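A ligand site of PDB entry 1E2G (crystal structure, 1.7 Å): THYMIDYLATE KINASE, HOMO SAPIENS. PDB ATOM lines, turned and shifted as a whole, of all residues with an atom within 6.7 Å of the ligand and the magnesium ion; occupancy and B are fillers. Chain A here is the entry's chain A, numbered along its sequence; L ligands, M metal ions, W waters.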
ATOM      1  N   GLY A  16       1.365  21.763  -8.670  1.00  0.00           N
ATOM      2  CA  GLY A  16       2.720  21.283  -8.793  1.00  0.00           C
ATOM      3  C   GLY A  16       2.788  20.386 -10.056  1.00  0.00           C
ATOM      4  O   GLY A  16       1.738  19.986 -10.559  1.00  0.00           O
ATOM      5  N   VAL A  17       4.017  20.140 -10.469  1.00  0.00           N
ATOM      6  CA  VAL A  17       4.185  19.279 -11.660  1.00  0.00           C
ATOM      7  C   VAL A  17       3.786  17.870 -11.326  1.00  0.00           C
ATOM      8  O   VAL A  17       3.464  17.561 -10.165  1.00  0.00           O
ATOM      9  CB  VAL A  17       5.662  19.405 -12.117  1.00  0.00           C
ATOM     10  CG1 VAL A  17       5.918  20.860 -12.468  1.00  0.00           C
ATOM     11  CG2 VAL A  17       6.631  18.938 -11.032  1.00  0.00           C
ATOM     12  N   ASP A  18       3.822  16.947 -12.300  1.00  0.00           N
ATOM     13  CA  ASP A  18       3.493  15.557 -11.966  1.00  0.00           C
ATOM     14  C   ASP A  18       4.564  15.059 -10.982  1.00  0.00           C
ATOM     15  O   ASP A  18       5.730  15.437 -10.984  1.00  0.00           O
ATOM     16  CB  ASP A  18       3.458  14.729 -13.252  1.00  0.00           C
ATOM     17  CG  ASP A  18       2.422  15.178 -14.260  1.00  0.00           C
ATOM     18  OD1 ASP A  18       1.360  15.682 -13.876  1.00  0.00           O
ATOM     19  OD2 ASP A  18       2.579  15.031 -15.495  1.00  0.00           O
ATOM     20  N   ARG A  19       4.151  14.216 -10.043  1.00  0.00           N
ATOM     21  CA  ARG A  19       4.904  13.535  -9.004  1.00  0.00           C
ATOM     22  C   ARG A  19       5.374  14.433  -7.865  1.00  0.00           C
ATOM     23  O   ARG A  19       6.241  14.063  -7.071  1.00  0.00           O
ATOM     24  CB  ARG A  19       6.072  12.685  -9.521  1.00  0.00           C
ATOM     25  CG  ARG A  19       5.797  11.958 -10.814  1.00  0.00           C
ATOM     26  CD  ARG A  19       4.363  11.528 -10.991  1.00  0.00           C
ATOM     27  NE  ARG A  19       4.113  10.245 -10.368  1.00  0.00           N
ATOM     28  CZ  ARG A  19       2.910   9.820  -9.965  1.00  0.00           C
ATOM     29  NH1 ARG A  19       1.842  10.588 -10.111  1.00  0.00           N
ATOM     30  NH2 ARG A  19       2.895   8.606  -9.411  1.00  0.00           N
ATOM     31  N   ALA A  20       4.783  15.627  -7.800  1.00  0.00           N
ATOM     32  CA  ALA A  20       5.196  16.581  -6.757  1.00  0.00           C
ATOM     33  C   ALA A  20       4.665  16.178  -5.381  1.00  0.00           C
ATOM     34  O   ALA A  20       5.095  16.736  -4.375  1.00  0.00           O
ATOM     35  CB  ALA A  20       4.638  17.960  -7.113  1.00  0.00           C
ATOM     36  N   GLY A  21       3.688  15.287  -5.374  1.00  0.00           N
ATOM     37  CA  GLY A  21       3.081  14.858  -4.112  1.00  0.00           C
ATOM     38  C   GLY A  21       1.685  15.454  -3.926  1.00  0.00           C
ATOM     39  O   GLY A  21       1.161  15.386  -2.807  1.00  0.00           O
ATOM     40  N   LYS A  22       1.038  16.042  -4.921  1.00  0.00           N
ATOM     41  CA  LYS A  22      -0.279  16.630  -4.821  1.00  0.00           C
ATOM     42  C   LYS A  22      -1.362  15.695  -4.271  1.00  0.00           C
ATOM     43  O   LYS A  22      -2.125  16.049  -3.388  1.00  0.00           O
ATOM     44  CB  LYS A  22      -0.784  17.194  -6.180  1.00  0.00           C
ATOM     45  CG  LYS A  22       0.298  18.179  -6.692  1.00  0.00           C
ATOM     46  CD  LYS A  22      -0.158  18.792  -8.028  1.00  0.00           C
ATOM     47  CE  LYS A  22      -0.444  17.749  -9.105  1.00  0.00           C
ATOM     48  NZ  LYS A  22       0.799  17.038  -9.495  1.00  0.00           N
ATOM     49  N   SER A  23      -1.501  14.519  -4.826  1.00  0.00           N
ATOM     50  CA  SER A  23      -2.563  13.600  -4.431  1.00  0.00           C
ATOM     51  C   SER A  23      -2.259  13.061  -3.026  1.00  0.00           C
ATOM     52  O   SER A  23      -3.187  12.959  -2.217  1.00  0.00           O
ATOM     53  CB  SER A  23      -2.646  12.466  -5.444  1.00  0.00           C
ATOM     54  OG  SER A  23      -3.012  13.028  -6.727  1.00  0.00           O
ATOM     55  N   THR A  24      -1.000  12.760  -2.770  1.00  0.00           N
ATOM     56  CA  THR A  24      -0.671  12.237  -1.414  1.00  0.00           C
ATOM     57  C   THR A  24      -0.993  13.304  -0.359  1.00  0.00           C
ATOM     58  O   THR A  24      -1.669  13.056   0.652  1.00  0.00           O
ATOM     59  CB  THR A  24       0.823  11.890  -1.303  1.00  0.00           C
ATOM     60  OG1 THR A  24       1.125  10.815  -2.210  1.00  0.00           O
ATOM     61  CG2 THR A  24       1.158  11.436   0.127  1.00  0.00           C
ATOM     62  N   GLN A  25      -0.549  14.537  -0.653  1.00  0.00           N
ATOM     63  CA  GLN A  25      -0.815  15.618   0.317  1.00  0.00           C
ATOM     64  C   GLN A  25      -2.279  16.005   0.393  1.00  0.00           C
ATOM     65  O   GLN A  25      -2.776  16.404   1.460  1.00  0.00           O
ATOM     66  CB  GLN A  25       0.131  16.798   0.037  1.00  0.00           C
ATOM     67  CG  GLN A  25       1.604  16.476   0.241  1.00  0.00           C
ATOM     68  CD  GLN A  25       1.938  15.994   1.642  1.00  0.00           C
ATOM     69  OE1 GLN A  25       1.243  16.319   2.622  1.00  0.00           O
ATOM     70  NE2 GLN A  25       2.975  15.171   1.764  1.00  0.00           N
ATOM     71  N   ARG A  27      -4.860  14.019   0.002  1.00  0.00           N
ATOM     72  CA  ARG A  27      -5.513  12.990   0.826  1.00  0.00           C
ATOM     73  C   ARG A  27      -5.184  13.137   2.320  1.00  0.00           C
ATOM     74  O   ARG A  27      -6.109  13.101   3.139  1.00  0.00           O
ATOM     75  CB  ARG A  27      -5.081  11.555   0.437  1.00  0.00           C
ATOM     76  CG  ARG A  27      -5.593  11.151  -0.942  1.00  0.00           C
ATOM     77  CD  ARG A  27      -5.283   9.661  -1.178  1.00  0.00           C
ATOM     78  NE  ARG A  27      -3.867   9.369  -1.142  1.00  0.00           N
ATOM     79  CZ  ARG A  27      -2.989   9.348  -2.142  1.00  0.00           C
ATOM     80  NH1 ARG A  27      -3.377   9.608  -3.392  1.00  0.00           N
ATOM     81  NH2 ARG A  27      -1.737   9.027  -1.879  1.00  0.00           N
ATOM     82  N   ASP A  99      -7.187  18.825  -5.635  1.00  0.00           N
ATOM     83  CA  ASP A  99      -6.004  18.259  -6.235  1.00  0.00           C
ATOM     84  C   ASP A  99      -5.939  18.587  -7.719  1.00  0.00           C
ATOM     85  O   ASP A  99      -6.617  17.880  -8.491  1.00  0.00           O
ATOM     86  CB  ASP A  99      -6.084  16.743  -6.038  1.00  0.00           C
ATOM     87  CG  ASP A  99      -4.834  16.023  -6.464  1.00  0.00           C
ATOM     88  OD1 ASP A  99      -3.837  16.508  -7.025  1.00  0.00           O
ATOM     89  OD2 ASP A  99      -4.956  14.750  -6.309  1.00  0.00           O
ATOM     90  N   ARG A 100      -5.229  19.643  -8.018  1.00  0.00           N
ATOM     91  CA  ARG A 100      -5.121  20.312  -9.291  1.00  0.00           C
ATOM     92  C   ARG A 100      -6.353  21.170  -9.594  1.00  0.00           C
ATOM     93  O   ARG A 100      -7.487  20.851  -9.235  1.00  0.00           O
ATOM     94  CB  ARG A 100      -4.840  19.443 -10.526  1.00  0.00           C
ATOM     95  CG  ARG A 100      -3.605  18.545 -10.324  1.00  0.00           C
ATOM     96  CD  ARG A 100      -3.312  17.772 -11.617  1.00  0.00           C
ATOM     97  NE  ARG A 100      -4.235  16.662 -11.808  1.00  0.00           N
ATOM     98  CZ  ARG A 100      -3.877  15.397 -12.074  1.00  0.00           C
ATOM     99  NH1 ARG A 100      -2.582  15.102 -12.157  1.00  0.00           N
ATOM    100  NH2 ARG A 100      -4.761  14.423 -12.257  1.00  0.00           N
ATOM    101  N   LEU A 136       3.560  22.864  -4.672  1.00  0.00           N
ATOM    102  CA  LEU A 136       4.536  21.869  -4.170  1.00  0.00           C
ATOM    103  C   LEU A 136       5.788  21.871  -5.015  1.00  0.00           C
ATOM    104  O   LEU A 136       5.876  21.281  -6.083  1.00  0.00           O
ATOM    105  CB  LEU A 136       3.828  20.513  -4.171  1.00  0.00           C
ATOM    106  CG  LEU A 136       3.021  20.266  -2.875  1.00  0.00           C
ATOM    107  CD1 LEU A 136       1.872  21.225  -2.670  1.00  0.00           C
ATOM    108  CD2 LEU A 136       2.475  18.835  -2.974  1.00  0.00           C
ATOM    109  N   ALA A 143      11.291  14.804  -8.817  1.00  0.00           N
ATOM    110  CA  ALA A 143       9.966  14.339  -9.230  1.00  0.00           C
ATOM    111  C   ALA A 143      10.086  13.111 -10.123  1.00  0.00           C
ATOM    112  O   ALA A 143       9.283  12.169 -10.050  1.00  0.00           O
ATOM    113  CB  ALA A 143       9.216  15.473  -9.896  1.00  0.00           C
ATOM    114  N   ARG A 146      10.349   9.415  -8.501  1.00  0.00           N
ATOM    115  CA  ARG A 146       9.145   8.881  -7.885  1.00  0.00           C
ATOM    116  C   ARG A 146       8.199   8.182  -8.845  1.00  0.00           C
ATOM    117  O   ARG A 146       8.252   8.424 -10.050  1.00  0.00           O
ATOM    118  CB  ARG A 146       8.391  10.080  -7.244  1.00  0.00           C
ATOM    119  CG  ARG A 146       9.246  10.848  -6.258  1.00  0.00           C
ATOM    120  CD  ARG A 146       8.451  12.094  -5.791  1.00  0.00           C
ATOM    121  NE  ARG A 146       9.090  12.814  -4.721  1.00  0.00           N
ATOM    122  CZ  ARG A 146       8.610  13.820  -3.994  1.00  0.00           C
ATOM    123  NH1 ARG A 146       7.407  14.311  -4.254  1.00  0.00           N
ATOM    124  NH2 ARG A 146       9.327  14.353  -3.034  1.00  0.00           N
ATOM    125  N   GLY A 147       7.275   7.344  -8.348  1.00  0.00           N
ATOM    126  CA  GLY A 147       6.285   6.692  -9.199  1.00  0.00           C
ATOM    127  C   GLY A 147       6.917   5.809 -10.281  1.00  0.00           C
ATOM    128  O   GLY A 147       7.982   5.232 -10.025  1.00  0.00           O
ATOM    129  N   ALA A 183       8.440  20.558  -1.278  1.00  0.00           N
ATOM    130  CA  ALA A 183       7.924  19.188  -1.452  1.00  0.00           C
ATOM    131  C   ALA A 183       8.989  18.132  -1.520  1.00  0.00           C
ATOM    132  O   ALA A 183       8.697  16.979  -1.775  1.00  0.00           O
ATOM    133  CB  ALA A 183       7.054  19.260  -2.709  1.00  0.00           C
ATOM    134  N   SER A 184      10.244  18.566  -1.342  1.00  0.00           N
ATOM    135  CA  SER A 184      11.352  17.599  -1.391  1.00  0.00           C
ATOM    136  C   SER A 184      11.520  16.895  -0.059  1.00  0.00           C
ATOM    137  O   SER A 184      12.242  15.878   0.033  1.00  0.00           O
ATOM    138  CB  SER A 184      12.660  18.318  -1.807  1.00  0.00           C
ATOM    139  OG  SER A 184      13.169  19.060  -0.699  1.00  0.00           O
ATOM    140  N   LYS A 185      10.884  17.351   1.006  1.00  0.00           N
ATOM    141  CA  LYS A 185      11.003  16.718   2.322  1.00  0.00           C
ATOM    142  C   LYS A 185      10.155  15.467   2.427  1.00  0.00           C
ATOM    143  O   LYS A 185       9.551  15.075   1.446  1.00  0.00           O
ATOM    144  CB  LYS A 185      10.589  17.734   3.396  1.00  0.00           C
ATOM    145  CG  LYS A 185      11.333  19.059   3.168  1.00  0.00           C
ATOM    146  CD  LYS A 185      11.228  19.979   4.369  1.00  0.00           C
ATOM    147  CE  LYS A 185       9.851  20.565   4.625  1.00  0.00           C
ATOM    148  NZ  LYS A 185       9.871  21.668   5.658  1.00  0.00           N
ATOM    149  N   SER A 186      10.166  14.842   3.610  1.00  0.00           N
ATOM    150  CA  SER A 186       9.434  13.585   3.763  1.00  0.00           C
ATOM    151  C   SER A 186       7.923  13.796   3.638  1.00  0.00           C
ATOM    152  O   SER A 186       7.464  14.937   3.813  1.00  0.00           O
ATOM    153  CB  SER A 186       9.697  12.994   5.144  1.00  0.00           C
ATOM    154  OG  SER A 186       9.097  13.701   6.202  1.00  0.00           O
ATOM    155  N   ILE A 187       7.181  12.722   3.384  1.00  0.00           N
ATOM    156  CA  ILE A 187       5.724  12.904   3.292  1.00  0.00           C
ATOM    157  C   ILE A 187       5.152  13.554   4.538  1.00  0.00           C
ATOM    158  O   ILE A 187       4.288  14.441   4.453  1.00  0.00           O
ATOM    159  CB  ILE A 187       5.075  11.528   3.006  1.00  0.00           C
ATOM    160  CG1 ILE A 187       5.441  11.121   1.571  1.00  0.00           C
ATOM    161  CG2 ILE A 187       3.585  11.560   3.267  1.00  0.00           C
ATOM    162  CD1 ILE A 187       4.804   9.780   1.237  1.00  0.00           C
ATOM    163  N   GLU A 188       5.624  13.117   5.720  1.00  0.00           N
ATOM    164  CA  GLU A 188       5.096  13.684   6.954  1.00  0.00           C
ATOM    165  C   GLU A 188       5.505  15.136   7.161  1.00  0.00           C
ATOM    166  O   GLU A 188       4.658  15.910   7.651  1.00  0.00           O
ATOM    167  CB  GLU A 188       5.581  12.836   8.141  1.00  0.00           C
ATOM    168  CG  GLU A 188       4.862  11.501   8.248  1.00  0.00           C
ATOM    169  CD  GLU A 188       3.347  11.655   8.360  1.00  0.00           C
ATOM    170  OE1 GLU A 188       2.855  12.600   9.034  1.00  0.00           O
ATOM    171  OE2 GLU A 188       2.656  10.808   7.751  1.00  0.00           O
ATOM    172  N   VAL A 190       6.252  17.350   4.795  1.00  0.00           N
ATOM    173  CA  VAL A 190       5.534  18.239   3.853  1.00  0.00           C
ATOM    174  C   VAL A 190       4.101  18.411   4.341  1.00  0.00           C
ATOM    175  O   VAL A 190       3.513  19.475   4.286  1.00  0.00           O
ATOM    176  CB  VAL A 190       5.577  17.576   2.469  1.00  0.00           C
ATOM    177  CG1 VAL A 190       4.754  18.356   1.450  1.00  0.00           C
ATOM    178  CG2 VAL A 190       7.046  17.533   1.995  1.00  0.00           C
HETATM  179  P1  LIG L   1       1.214  13.784  -7.743  1.00  0.00           P
HETATM  180  O1  LIG L   1       1.782  15.182  -7.583  1.00  0.00           O
HETATM  181  O2  LIG L   1      -0.197  13.656  -7.548  1.00  0.00           O
HETATM  182  O3  LIG L   1       1.646  13.171  -9.148  1.00  0.00           O
HETATM  183  P2  LIG L   1       1.734  11.641  -5.787  1.00  0.00           P
HETATM  184  O4  LIG L   1       0.794  10.729  -6.476  1.00  0.00           O
HETATM  185  O5  LIG L   1       1.134  12.177  -4.491  1.00  0.00           O
HETATM  186  O6  LIG L   1       2.121  12.914  -6.716  1.00  0.00           O
HETATM  187  O7  LIG L   1       3.125  11.050  -5.491  1.00  0.00           O
HETATM  188  C1  LIG L   1       3.903  10.431  -6.588  1.00  0.00           C
HETATM  189  C2  LIG L   1       4.757   9.323  -5.963  1.00  0.00           C
HETATM  190  O8  LIG L   1       5.732   9.905  -5.130  1.00  0.00           O
HETATM  191  C3  LIG L   1       3.955   8.326  -5.157  1.00  0.00           C
HETATM  192  O9  LIG L   1       4.526   7.019  -5.243  1.00  0.00           O
HETATM  193  C4  LIG L   1       4.221   8.838  -3.735  1.00  0.00           C
HETATM  194  O10 LIG L   1       4.192   7.875  -2.713  1.00  0.00           O
HETATM  195  C5  LIG L   1       5.632   9.404  -3.826  1.00  0.00           C
HETATM  196  N1  LIG L   1       5.799  10.575  -2.939  1.00  0.00           N
HETATM  197  C6  LIG L   1       4.844  11.533  -2.637  1.00  0.00           C
HETATM  198  N2  LIG L   1       5.317  12.431  -1.782  1.00  0.00           N
HETATM  199  C7  LIG L   1       6.637  12.033  -1.531  1.00  0.00           C
HETATM  200  C8  LIG L   1       7.621  12.584  -0.728  1.00  0.00           C
HETATM  201  N3  LIG L   1       7.467  13.637   0.013  1.00  0.00           N
HETATM  202  N4  LIG L   1       8.794  11.918  -0.796  1.00  0.00           N
HETATM  203  C9  LIG L   1       9.024  10.838  -1.554  1.00  0.00           C
HETATM  204  N5  LIG L   1       8.113  10.253  -2.338  1.00  0.00           N
HETATM  205  C10 LIG L   1       6.980  10.911  -2.249  1.00  0.00           C
HETATM  206 MG    MG M   1      -1.883  12.995  -8.458  1.00  0.00          MG
HETATM  207  O   HOH W   1       3.396   6.446  -7.569  1.00  0.00           O
HETATM  208  O   HOH W   2       8.274   8.407   0.792  1.00  0.00           O
HETATM  209  O   HOH W   3      -3.671  12.228  -9.395  1.00  0.00           O
HETATM  210  O   HOH W   4       1.833   8.138  -1.929  1.00  0.00           O
HETATM  211  O   HOH W   5      -2.848  15.014  -8.775  1.00  0.00           O
HETATM  212  O   HOH W   6       0.872   8.050  -7.387  1.00  0.00           O
HETATM  213  O   HOH W   7       6.382   7.097  -1.081  1.00  0.00           O
HETATM  214  O   HOH W   8      -0.939  12.961 -10.344  1.00  0.00           O
HETATM  215  O   HOH W   9       9.138   7.946  -3.781  1.00  0.00           O
HETATM  216  O   HOH W  10      -1.204  11.029  -8.066  1.00  0.00           O
HETATM  217  O   HOH W  11       7.941   6.779  -5.814  1.00  0.00           O
HETATM  218  O   HOH W  12      11.248  12.818   0.199  1.00  0.00           O
HETATM  219  O   HOH W  13       4.653  14.718  -0.442  1.00  0.00           O
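An oxygen (O1) of the ligand is in hydrogen-bond range of the backbone NH of Ala 20, at 3.0 Å. The side-chain hydroxyl (OG1) of Thr 24 lies within hydrogen-bond range of an oxygen (O5) of the ligand (2.7 Å). The backbone NH (N) of Gly 21 lies within hydrogen-bond range of an oxygen (O1) of the ligand, 2.9 Å away. The guanidinium group of Arg 146 is in hydrogen-bond range of a nitrogen (N4) of the ligand (3.3 Å). N of Lys 22 is in hydrogen-bond range of O1 of the ligand (2.9 Å). The backbone NH of Arg 19 is in hydrogen-bond range of an oxygen (O3) of the ligand, at 2.9 Å. An oxygen (O3) of the ligand lies within salt-bridge range of the guanidinium group of Arg 19. N of Thr 24 is in hydrogen-bond range of O5 of the ligand, 2.8 Å away. The side-chain amino group of Lys 22 is in salt-bridge range of an oxygen (O1) of the ligand (2.8 Å). O of Lys 185 sits at hydrogen-bond distance from N3 of the ligand, 2.9 Å away. N of Ser 23 sits close to O2 of the ligand, at 3.1 Å.
The guanidinium group (NH2) of Arg 146 sits at hydrogen-bond distance from the backbone carbonyl oxygen (O) of Ala 183 (3.0 Å). The side-chain amino group (NZ) of Lys 22 sits at hydrogen-bond distance from the backbone carbonyl oxygen (O) of Gly 16, at 3.3 Å. OG1 of Thr 24 is in hydrogen-bond range of NH2 of Arg 27, 3.4 Å away. O of Ile 187 sits at hydrogen-bond distance from NE2 of Gln 25 (3.1 Å). The side-chain hydroxyl (OG) of Ser 23 lies close to the side-chain carboxylate (OD2) of Asp 99 (2.6 Å). O of Val 17 sits at hydrogen-bond distance from NZ of Lys 22, 2.8 Å away. O of Ala 20 sits at hydrogen-bond distance from NH1 of Arg 146, at 3.4 Å. O of Arg 19 sits at hydrogen-bond distance from NH1 of Arg 146 (3.1 Å).
O of Val 17 touches O1 of the ligand, 3.9 Å away. C of Asp 18 touches O3 of the ligand, 3.9 Å away. Gly 147 touches the ligand. Ala 183 touches the ligand. Ser 186 touches the ligand (C to N3, 3.7 Å). Ile 187 touches the ligand (CG1 to C7, 3.4 Å). Hydrophobic or aromatic side chains that line the ligand: Ile 187.
Within 4 Å of the magnesium ion: Ser 23.
The magnesium ion is bound by O2 of the ligand, OG of Ser 23, water W8, water W10, water W3 and water W5. The magnesium ion has six donor atoms within binding distance.
Water W5 lies within hydrogen-bond range of the side-chain carboxylate of Asp 99 and the guanidinium group of Arg 100. Water W4 lies within hydrogen-bond range of an oxygen (O10) of the ligand (2.5 Å) and the side-chain hydroxyl of Thr 24 (2.8 Å). Water W1 bridges an oxygen (O9) of the ligand (2.6 Å) and the guanidinium group (NH2) of Arg 19 (2.9 Å). Water W13 lies within hydrogen-bond range of a nitrogen (N2) of the ligand and the side-chain amide nitrogen of Gln 25. Water W6 bridges an oxygen (O4) of the ligand (2.8 Å) and the guanidinium group (NH2) of Arg 19 (2.9 Å). Water W11 lies within hydrogen-bond range of the backbone NH of Gly 147 (2.7 Å) and an oxygen (O9) of the ligand (3.5 Å).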
